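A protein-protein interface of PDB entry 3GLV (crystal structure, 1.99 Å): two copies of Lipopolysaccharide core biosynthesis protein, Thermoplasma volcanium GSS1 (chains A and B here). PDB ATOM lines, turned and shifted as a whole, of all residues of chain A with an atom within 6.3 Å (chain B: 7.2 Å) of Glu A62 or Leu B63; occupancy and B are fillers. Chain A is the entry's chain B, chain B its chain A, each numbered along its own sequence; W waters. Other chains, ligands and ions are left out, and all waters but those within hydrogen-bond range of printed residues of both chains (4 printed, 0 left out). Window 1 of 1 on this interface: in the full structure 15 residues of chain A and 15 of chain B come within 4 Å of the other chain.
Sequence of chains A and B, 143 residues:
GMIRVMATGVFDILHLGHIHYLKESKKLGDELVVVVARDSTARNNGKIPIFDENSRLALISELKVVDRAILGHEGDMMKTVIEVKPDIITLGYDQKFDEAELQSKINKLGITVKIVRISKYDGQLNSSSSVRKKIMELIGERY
Of chain B, only Ile B19 (3.7 Å), Lys B23 (2.6 Å), Leu B63 (3.4 Å) and Lys B64 (2.8 Å) come within 4 Å of Glu A62.
Leu B63 touches just these residues of chain A: Glu A62 (3.4 Å) and Lys A64 (2.9 Å).
Of the printed residues of chain A, Val B66 touches Lys A64 (3.0 Å).
Of the printed residues of chain B, Leu A59 touches Leu B14 (3.4 Å) and Ile B19 (3.4 Å).
Of the printed residues of chain B, Leu A14 touches Leu B59 (3.4 Å).
Printed residues of chain A within 4 Å of Leu B14: Leu A59 (3.4 Å).
Hydrophobic or aromatic side chains of chain A within 4 Å of the printed part of chain B: Ala A58, Leu A59 and Leu A63.
Printed residues of chain B that touch a printed residue of chain A: Leu B14, Leu B16, Ile B19, Lys B23, Leu B59, Ser B61, Glu B62, Leu B63, Lys B64 and Val B66.
Among the printed residues, Asp or Glu carboxylates within 4 Å of a Lys or Arg side-chain nitrogen of the other chain: Glu A62 with Lys B23.
Leu A14 touches Leu B59.
CD2 of Leu B16 touches CB of Ala A58 (3.8 Å).
CD2 of Leu A59 touches O of Leu B14 (3.4 Å).
CD1 of Leu A59 touches CG1 of Ile B19, 3.4 Å away.
Ser A61 touches Lys B64 (O to CE, 3.4 Å).
CG2 of Ile B19 touches CG of Glu A62, at 3.7 Å.
Glu A62 touches Leu B63 (O to CA, 3.4 Å).
O of Glu B62 touches CA of Leu A63, at 3.5 Å.
Lys A64 touches Ser B61.
The backbone carbonyl oxygen (O) of Leu A57 sits at hydrogen-bond distance from the side-chain hydroxyl (OG) of Ser A61.
OE2 of Glu A62 is in salt-bridge range of NZ of Lys B23 (2.6 Å).
The backbone NH (N) of Lys A64 lies within hydrogen-bond range of the backbone carbonyl oxygen (O) of Glu B62, at 2.8 Å.
The side-chain amino group of Lys A64 sits at hydrogen-bond distance from the backbone carbonyl oxygen of Leu B63 (2.9 Å).
N of Lys B64 is in hydrogen-bond range of O of Glu A62, at 2.8 Å.
NZ of Lys B64 is in hydrogen-bond range of O of Leu A63 (2.7 Å).
The side-chain amino group (NZ) of Lys A64 is in hydrogen-bond range of the backbone carbonyl oxygen (O) of Lys B64 (3.0 Å).
The backbone carbonyl oxygen (O) of Val A66 lies within hydrogen-bond range of the side-chain amino group (NZ) of Lys B64, 2.9 Å away.
The backbone carbonyl oxygen (O) of Val B66 lies within hydrogen-bond range of the side-chain amino group (NZ) of Lys A64 (3.0 Å).
Ser A61 touches Lys B64, and with the chains exchanged Lys A64 touches Ser B61.
Glu A62 touches Leu B63, and with the chains exchanged Leu A63 touches Glu B62.
Lys A64 touches its own counterpart, Lys B64.
Lys A64 touches Val B66, and with the chains exchanged Val A66 touches Lys B64.
9 positions are printed for both chains.
Of the 17 pairs that touch across the chains among the printed residues, 13 have their exchanged pair printed and touching as well.
Water W2 lies within hydrogen-bond range of the side-chain carboxylate (OE1) of Glu B62 and the backbone NH (N) of Lys A64.
Water W3 lies within hydrogen-bond range of the backbone carbonyl oxygen of Glu A62 (2.7 Å), the backbone NH of Lys B64 (2.9 Å) and the backbone NH of Val B65 (3.1 Å).
Water W1 bridges N of Leu B14 (2.9 Å) and O of Leu A14 (2.9 Å).
Water W4 lies within hydrogen-bond range of the backbone carbonyl oxygen (O) of Leu B14 (2.9 Å) and the backbone NH (N) of Leu A14 (2.9 Å).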
ATOM      1  N   LEU A  14      36.999  13.291 -18.494  1.00  0.00           N
ATOM      2  CA  LEU A  14      36.506  14.267 -19.442  1.00  0.00           C
ATOM      3  C   LEU A  14      37.306  15.577 -19.316  1.00  0.00           C
ATOM      4  O   LEU A  14      37.590  16.060 -18.223  1.00  0.00           O
ATOM      5  CB  LEU A  14      35.030  14.583 -19.229  1.00  0.00           C
ATOM      6  CG  LEU A  14      33.908  13.803 -19.891  1.00  0.00           C
ATOM      7  CD1 LEU A  14      32.705  14.700 -19.746  1.00  0.00           C
ATOM      8  CD2 LEU A  14      34.201  13.462 -21.372  1.00  0.00           C
ATOM      9  N   LEU A  57      30.157   5.935 -20.503  1.00  0.00           N
ATOM     10  CA  LEU A  57      29.055   6.094 -21.474  1.00  0.00           C
ATOM     11  C   LEU A  57      28.004   7.092 -20.962  1.00  0.00           C
ATOM     12  O   LEU A  57      27.605   8.014 -21.680  1.00  0.00           O
ATOM     13  CB  LEU A  57      28.390   4.730 -21.785  1.00  0.00           C
ATOM     14  CG  LEU A  57      27.161   4.743 -22.704  1.00  0.00           C
ATOM     15  CD1 LEU A  57      27.549   5.256 -24.074  1.00  0.00           C
ATOM     16  CD2 LEU A  57      26.567   3.332 -22.835  1.00  0.00           C
ATOM     17  N   ALA A  58      27.607   6.930 -19.704  1.00  0.00           N
ATOM     18  CA  ALA A  58      26.586   7.772 -19.096  1.00  0.00           C
ATOM     19  C   ALA A  58      27.020   9.212 -18.986  1.00  0.00           C
ATOM     20  O   ALA A  58      26.236  10.134 -19.225  1.00  0.00           O
ATOM     21  CB  ALA A  58      26.199   7.227 -17.707  1.00  0.00           C
ATOM     22  N   LEU A  59      28.276   9.440 -18.640  1.00  0.00           N
ATOM     23  CA  LEU A  59      28.762  10.788 -18.571  1.00  0.00           C
ATOM     24  C   LEU A  59      28.821  11.427 -19.941  1.00  0.00           C
ATOM     25  O   LEU A  59      28.414  12.550 -20.115  1.00  0.00           O
ATOM     26  CB  LEU A  59      30.133  10.813 -17.891  1.00  0.00           C
ATOM     27  CG  LEU A  59      30.689  12.118 -17.413  1.00  0.00           C
ATOM     28  CD1 LEU A  59      29.617  12.957 -16.661  1.00  0.00           C
ATOM     29  CD2 LEU A  59      31.897  11.856 -16.502  1.00  0.00           C
ATOM     30  N   ILE A  60      29.302  10.715 -20.932  1.00  0.00           N
ATOM     31  CA  ILE A  60      29.364  11.275 -22.289  1.00  0.00           C
ATOM     32  C   ILE A  60      27.949  11.671 -22.796  1.00  0.00           C
ATOM     33  O   ILE A  60      27.773  12.672 -23.507  1.00  0.00           O
ATOM     34  CB  ILE A  60      29.998  10.203 -23.195  1.00  0.00           C
ATOM     35  CG1 ILE A  60      31.474  10.445 -23.324  1.00  0.00           C
ATOM     36  CG2 ILE A  60      29.335  10.122 -24.582  1.00  0.00           C
ATOM     37  CD1 ILE A  60      31.860  11.748 -23.988  1.00  0.00           C
ATOM     38  N   SER A  61      26.936  10.888 -22.399  1.00  0.00           N
ATOM     39  CA  SER A  61      25.551  11.088 -22.793  1.00  0.00           C
ATOM     40  C   SER A  61      24.959  12.371 -22.229  1.00  0.00           C
ATOM     41  O   SER A  61      23.950  12.846 -22.757  1.00  0.00           O
ATOM     42  CB  SER A  61      24.673   9.926 -22.318  1.00  0.00           C
ATOM     43  OG  SER A  61      25.154   8.737 -22.908  1.00  0.00           O
ATOM     44  N   GLU A  62      25.610  12.951 -21.207  1.00  0.00           N
ATOM     45  CA  GLU A  62      25.134  14.155 -20.548  1.00  0.00           C
ATOM     46  C   GLU A  62      25.589  15.430 -21.214  1.00  0.00           C
ATOM     47  O   GLU A  62      25.250  16.541 -20.742  1.00  0.00           O
ATOM     48  CB  GLU A  62      25.578  14.154 -19.066  1.00  0.00           C
ATOM     49  CG  GLU A  62      24.863  13.050 -18.212  1.00  0.00           C
ATOM     50  CD  GLU A  62      23.350  13.211 -18.100  1.00  0.00           C
ATOM     51  OE1 GLU A  62      22.840  14.330 -18.119  1.00  0.00           O
ATOM     52  OE2 GLU A  62      22.617  12.212 -17.941  1.00  0.00           O
ATOM     53  N   LEU A  63      26.419  15.307 -22.235  1.00  0.00           N
ATOM     54  CA  LEU A  63      26.911  16.492 -22.943  1.00  0.00           C
ATOM     55  C   LEU A  63      25.948  17.035 -23.970  1.00  0.00           C
ATOM     56  O   LEU A  63      25.337  16.267 -24.773  1.00  0.00           O
ATOM     57  CB  LEU A  63      28.221  16.191 -23.624  1.00  0.00           C
ATOM     58  CG  LEU A  63      29.389  15.888 -22.694  1.00  0.00           C
ATOM     59  CD1 LEU A  63      30.545  15.360 -23.537  1.00  0.00           C
ATOM     60  CD2 LEU A  63      29.783  17.088 -21.810  1.00  0.00           C
ATOM     61  N   LYS A  64      25.803  18.364 -23.962  1.00  0.00           N
ATOM     62  CA  LYS A  64      24.918  19.029 -24.901  1.00  0.00           C
ATOM     63  C   LYS A  64      25.198  18.577 -26.333  1.00  0.00           C
ATOM     64  O   LYS A  64      24.257  18.371 -27.100  1.00  0.00           O
ATOM     65  CB  LYS A  64      25.077  20.575 -24.829  1.00  0.00           C
ATOM     66  CG  LYS A  64      24.449  21.299 -23.590  1.00  0.00           C
ATOM     67  CD  LYS A  64      24.795  22.874 -23.572  1.00  0.00           C
ATOM     68  CE  LYS A  64      24.434  23.537 -22.234  1.00  0.00           C
ATOM     69  NZ  LYS A  64      23.101  22.988 -21.622  1.00  0.00           N
ATOM     70  N   VAL A  66      26.278  15.844 -27.589  1.00  0.00           N
ATOM     71  CA  VAL A  66      26.131  14.428 -27.880  1.00  0.00           C
ATOM     72  C   VAL A  66      24.650  14.020 -28.042  1.00  0.00           C
ATOM     73  O   VAL A  66      23.876  14.139 -27.098  1.00  0.00           O
ATOM     74  CB  VAL A  66      26.775  13.533 -26.778  1.00  0.00           C
ATOM     75  CG1 VAL A  66      26.566  12.071 -27.082  1.00  0.00           C
ATOM     76  CG2 VAL A  66      28.273  13.858 -26.594  1.00  0.00           C
ATOM     77  N   PHE B  11      33.740  20.542  -8.870  1.00  0.00           N
ATOM     78  CA  PHE B  11      33.631  19.802 -10.133  1.00  0.00           C
ATOM     79  C   PHE B  11      34.988  19.615 -10.792  1.00  0.00           C
ATOM     80  O   PHE B  11      35.177  19.968 -11.944  1.00  0.00           O
ATOM     81  CB  PHE B  11      32.635  20.504 -11.105  1.00  0.00           C
ATOM     82  CG  PHE B  11      31.272  20.775 -10.471  1.00  0.00           C
ATOM     83  CD1 PHE B  11      30.401  19.712 -10.201  1.00  0.00           C
ATOM     84  CD2 PHE B  11      30.893  22.076 -10.077  1.00  0.00           C
ATOM     85  CE1 PHE B  11      29.165  19.937  -9.578  1.00  0.00           C
ATOM     86  CE2 PHE B  11      29.669  22.314  -9.451  1.00  0.00           C
ATOM     87  CZ  PHE B  11      28.810  21.225  -9.196  1.00  0.00           C
ATOM     88  N   LEU B  14      34.888  15.286 -13.375  1.00  0.00           N
ATOM     89  CA  LEU B  14      33.428  15.033 -13.459  1.00  0.00           C
ATOM     90  C   LEU B  14      33.140  13.566 -13.269  1.00  0.00           C
ATOM     91  O   LEU B  14      33.835  12.689 -13.836  1.00  0.00           O
ATOM     92  CB  LEU B  14      32.794  15.503 -14.781  1.00  0.00           C
ATOM     93  CG  LEU B  14      32.439  16.975 -14.973  1.00  0.00           C
ATOM     94  CD1 LEU B  14      31.834  17.293 -16.319  1.00  0.00           C
ATOM     95  CD2 LEU B  14      31.481  17.415 -13.817  1.00  0.00           C
ATOM     96  N   LEU B  16      29.611  10.643 -11.987  1.00  0.00           N
ATOM     97  CA  LEU B  16      28.169  10.470 -12.010  1.00  0.00           C
ATOM     98  C   LEU B  16      27.474  11.003 -10.740  1.00  0.00           C
ATOM     99  O   LEU B  16      26.257  11.258 -10.742  1.00  0.00           O
ATOM    100  CB  LEU B  16      27.775   9.010 -12.307  1.00  0.00           C
ATOM    101  CG  LEU B  16      27.933   8.621 -13.797  1.00  0.00           C
ATOM    102  CD1 LEU B  16      27.688   7.168 -14.046  1.00  0.00           C
ATOM    103  CD2 LEU B  16      27.022   9.440 -14.712  1.00  0.00           C
ATOM    104  N   HIS B  18      28.269  13.972  -9.499  1.00  0.00           N
ATOM    105  CA  HIS B  18      28.037  15.297  -9.886  1.00  0.00           C
ATOM    106  C   HIS B  18      26.792  15.311 -10.776  1.00  0.00           C
ATOM    107  O   HIS B  18      25.930  16.169 -10.628  1.00  0.00           O
ATOM    108  CB  HIS B  18      29.218  15.860 -10.702  1.00  0.00           C
ATOM    109  CG  HIS B  18      30.463  16.038  -9.923  1.00  0.00           C
ATOM    110  ND1 HIS B  18      31.680  15.599 -10.393  1.00  0.00           N
ATOM    111  CD2 HIS B  18      30.705  16.652  -8.727  1.00  0.00           C
ATOM    112  CE1 HIS B  18      32.621  15.922  -9.508  1.00  0.00           C
ATOM    113  NE2 HIS B  18      32.061  16.578  -8.501  1.00  0.00           N
ATOM    114  N   ILE B  19      26.739  14.426 -11.760  1.00  0.00           N
ATOM    115  CA  ILE B  19      25.608  14.369 -12.663  1.00  0.00           C
ATOM    116  C   ILE B  19      24.306  14.203 -11.870  1.00  0.00           C
ATOM    117  O   ILE B  19      23.290  14.855 -12.184  1.00  0.00           O
ATOM    118  CB  ILE B  19      25.727  13.207 -13.656  1.00  0.00           C
ATOM    119  CG1 ILE B  19      26.962  13.377 -14.570  1.00  0.00           C
ATOM    120  CG2 ILE B  19      24.433  13.088 -14.514  1.00  0.00           C
ATOM    121  CD1 ILE B  19      27.050  14.818 -15.232  1.00  0.00           C
ATOM    122  N   LEU B  22      23.478  17.657 -10.162  1.00  0.00           N
ATOM    123  CA  LEU B  22      23.051  18.623 -11.132  1.00  0.00           C
ATOM    124  C   LEU B  22      21.689  18.269 -11.765  1.00  0.00           C
ATOM    125  O   LEU B  22      20.820  19.069 -11.788  1.00  0.00           O
ATOM    126  CB  LEU B  22      24.129  18.831 -12.182  1.00  0.00           C
ATOM    127  CG  LEU B  22      25.459  19.378 -11.682  1.00  0.00           C
ATOM    128  CD1 LEU B  22      26.440  19.659 -12.797  1.00  0.00           C
ATOM    129  CD2 LEU B  22      25.219  20.609 -10.871  1.00  0.00           C
ATOM    130  N   LYS B  23      21.523  17.048 -12.234  1.00  0.00           N
ATOM    131  CA  LYS B  23      20.297  16.613 -12.863  1.00  0.00           C
ATOM    132  C   LYS B  23      19.107  16.717 -11.953  1.00  0.00           C
ATOM    133  O   LYS B  23      18.009  17.158 -12.392  1.00  0.00           O
ATOM    134  CB  LYS B  23      20.432  15.215 -13.427  1.00  0.00           C
ATOM    135  CG  LYS B  23      19.213  14.707 -14.099  1.00  0.00           C
ATOM    136  CD  LYS B  23      19.436  13.311 -14.806  1.00  0.00           C
ATOM    137  CE  LYS B  23      20.389  13.404 -16.019  1.00  0.00           C
ATOM    138  NZ  LYS B  23      20.307  12.094 -16.729  1.00  0.00           N
ATOM    139  N   VAL B  34      24.904  27.016 -12.134  1.00  0.00           N
ATOM    140  CA  VAL B  34      25.921  26.340 -11.315  1.00  0.00           C
ATOM    141  C   VAL B  34      27.027  27.275 -10.942  1.00  0.00           C
ATOM    142  O   VAL B  34      27.611  28.007 -11.838  1.00  0.00           O
ATOM    143  CB  VAL B  34      26.492  25.070 -12.034  1.00  0.00           C
ATOM    144  CG1 VAL B  34      27.574  24.402 -11.161  1.00  0.00           C
ATOM    145  CG2 VAL B  34      25.364  24.098 -12.417  1.00  0.00           C
ATOM    146  N   ALA B  58      34.175  25.823 -17.759  1.00  0.00           N
ATOM    147  CA  ALA B  58      33.879  25.520 -19.176  1.00  0.00           C
ATOM    148  C   ALA B  58      33.322  24.107 -19.367  1.00  0.00           C
ATOM    149  O   ALA B  58      32.369  23.897 -20.131  1.00  0.00           O
ATOM    150  CB  ALA B  58      35.125  25.723 -20.032  1.00  0.00           C
ATOM    151  N   LEU B  59      33.903  23.122 -18.677  1.00  0.00           N
ATOM    152  CA  LEU B  59      33.400  21.773 -18.810  1.00  0.00           C
ATOM    153  C   LEU B  59      32.002  21.671 -18.246  1.00  0.00           C
ATOM    154  O   LEU B  59      31.115  21.148 -18.930  1.00  0.00           O
ATOM    155  CB  LEU B  59      34.323  20.743 -18.152  1.00  0.00           C
ATOM    156  CG  LEU B  59      34.169  19.304 -18.548  1.00  0.00           C
ATOM    157  CD1 LEU B  59      34.176  19.023 -20.095  1.00  0.00           C
ATOM    158  CD2 LEU B  59      35.240  18.445 -17.806  1.00  0.00           C
ATOM    159  N   ILE B  60      31.774  22.179 -17.040  1.00  0.00           N
ATOM    160  CA  ILE B  60      30.403  22.164 -16.441  1.00  0.00           C
ATOM    161  C   ILE B  60      29.344  22.775 -17.397  1.00  0.00           C
ATOM    162  O   ILE B  60      28.226  22.294 -17.506  1.00  0.00           O
ATOM    163  CB  ILE B  60      30.400  22.914 -15.072  1.00  0.00           C
ATOM    164  CG1 ILE B  60      30.709  21.938 -13.947  1.00  0.00           C
ATOM    165  CG2 ILE B  60      29.054  23.594 -14.771  1.00  0.00           C
ATOM    166  CD1 ILE B  60      29.654  20.849 -13.803  1.00  0.00           C
ATOM    167  N   SER B  61      29.734  23.816 -18.133  1.00  0.00           N
ATOM    168  CA  SER B  61      28.843  24.526 -19.059  1.00  0.00           C
ATOM    169  C   SER B  61      28.417  23.640 -20.242  1.00  0.00           C
ATOM    170  O   SER B  61      27.507  24.006 -21.005  1.00  0.00           O
ATOM    171  CB  SER B  61      29.571  25.754 -19.648  1.00  0.00           C
ATOM    172  OG  SER B  61      29.739  26.661 -18.564  1.00  0.00           O
ATOM    173  N   GLU B  62      29.100  22.524 -20.440  1.00  0.00           N
ATOM    174  CA  GLU B  62      28.816  21.675 -21.597  1.00  0.00           C
ATOM    175  C   GLU B  62      27.763  20.639 -21.289  1.00  0.00           C
ATOM    176  O   GLU B  62      27.390  19.872 -22.198  1.00  0.00           O
ATOM    177  CB  GLU B  62      30.112  21.008 -22.114  1.00  0.00           C
ATOM    178  CG  GLU B  62      31.117  22.025 -22.741  1.00  0.00           C
ATOM    179  CD  GLU B  62      30.650  22.611 -24.045  1.00  0.00           C
ATOM    180  OE1 GLU B  62      29.844  21.951 -24.743  1.00  0.00           O
ATOM    181  OE2 GLU B  62      31.146  23.708 -24.410  1.00  0.00           O
ATOM    182  N   LEU B  63      27.293  20.577 -20.041  1.00  0.00           N
ATOM    183  CA  LEU B  63      26.256  19.617 -19.666  1.00  0.00           C
ATOM    184  C   LEU B  63      24.849  20.028 -20.036  1.00  0.00           C
ATOM    185  O   LEU B  63      24.420  21.176 -19.797  1.00  0.00           O
ATOM    186  CB  LEU B  63      26.282  19.329 -18.178  1.00  0.00           C
ATOM    187  CG  LEU B  63      27.616  18.770 -17.672  1.00  0.00           C
ATOM    188  CD1 LEU B  63      27.607  18.812 -16.150  1.00  0.00           C
ATOM    189  CD2 LEU B  63      27.850  17.372 -18.254  1.00  0.00           C
ATOM    190  N   LYS B  64      24.098  19.074 -20.590  1.00  0.00           N
ATOM    191  CA  LYS B  64      22.724  19.349 -21.036  1.00  0.00           C
ATOM    192  C   LYS B  64      21.937  20.081 -19.961  1.00  0.00           C
ATOM    193  O   LYS B  64      21.268  21.040 -20.259  1.00  0.00           O
ATOM    194  CB  LYS B  64      21.968  18.034 -21.389  1.00  0.00           C
ATOM    195  CG  LYS B  64      22.415  17.384 -22.730  1.00  0.00           C
ATOM    196  CD  LYS B  64      21.619  16.074 -23.066  1.00  0.00           C
ATOM    197  CE  LYS B  64      22.199  15.294 -24.284  1.00  0.00           C
ATOM    198  NZ  LYS B  64      22.736  16.183 -25.450  1.00  0.00           N
ATOM    199  N   VAL B  65      22.052  19.627 -18.710  1.00  0.00           N
ATOM    200  CA  VAL B  65      21.175  20.116 -17.665  1.00  0.00           C
ATOM    201  C   VAL B  65      21.574  21.490 -17.120  1.00  0.00           C
ATOM    202  O   VAL B  65      20.786  22.094 -16.396  1.00  0.00           O
ATOM    203  CB  VAL B  65      21.035  19.091 -16.495  1.00  0.00           C
ATOM    204  CG1 VAL B  65      20.512  17.758 -17.025  1.00  0.00           C
ATOM    205  CG2 VAL B  65      22.315  18.927 -15.719  1.00  0.00           C
ATOM    206  N   VAL B  66      22.744  22.018 -17.518  1.00  0.00           N
ATOM    207  CA  VAL B  66      23.218  23.264 -17.006  1.00  0.00           C
ATOM    208  C   VAL B  66      22.861  24.420 -17.940  1.00  0.00           C
ATOM    209  O   VAL B  66      23.342  24.511 -19.104  1.00  0.00           O
ATOM    210  CB  VAL B  66      24.774  23.257 -16.723  1.00  0.00           C
ATOM    211  CG1 VAL B  66      25.241  24.606 -16.223  1.00  0.00           C
ATOM    212  CG2 VAL B  66      25.161  22.156 -15.758  1.00  0.00           C
ATOM    213  N   ASP B  67      22.085  25.363 -17.411  1.00  0.00           N
ATOM    214  CA  ASP B  67      21.737  26.542 -18.222  1.00  0.00           C
ATOM    215  C   ASP B  67      22.825  27.592 -18.174  1.00  0.00           C
ATOM    216  O   ASP B  67      23.187  28.122 -19.219  1.00  0.00           O
ATOM    217  CB  ASP B  67      20.397  27.073 -17.810  1.00  0.00           C
ATOM    218  CG  ASP B  67      19.320  26.049 -18.046  1.00  0.00           C
ATOM    219  OD1 ASP B  67      19.151  25.703 -19.231  1.00  0.00           O
ATOM    220  OD2 ASP B  67      18.745  25.509 -17.079  1.00  0.00           O
HETATM  221  O   HOH W   1      36.521  16.163 -15.543  1.00  0.00           O
HETATM  222  O   HOH W   2      28.499  19.675 -24.880  1.00  0.00           O
HETATM  223  O   HOH W   3      23.752  17.035 -18.559  1.00  0.00           O
HETATM  224  O   HOH W   4      35.473  12.349 -16.182  1.00  0.00           O
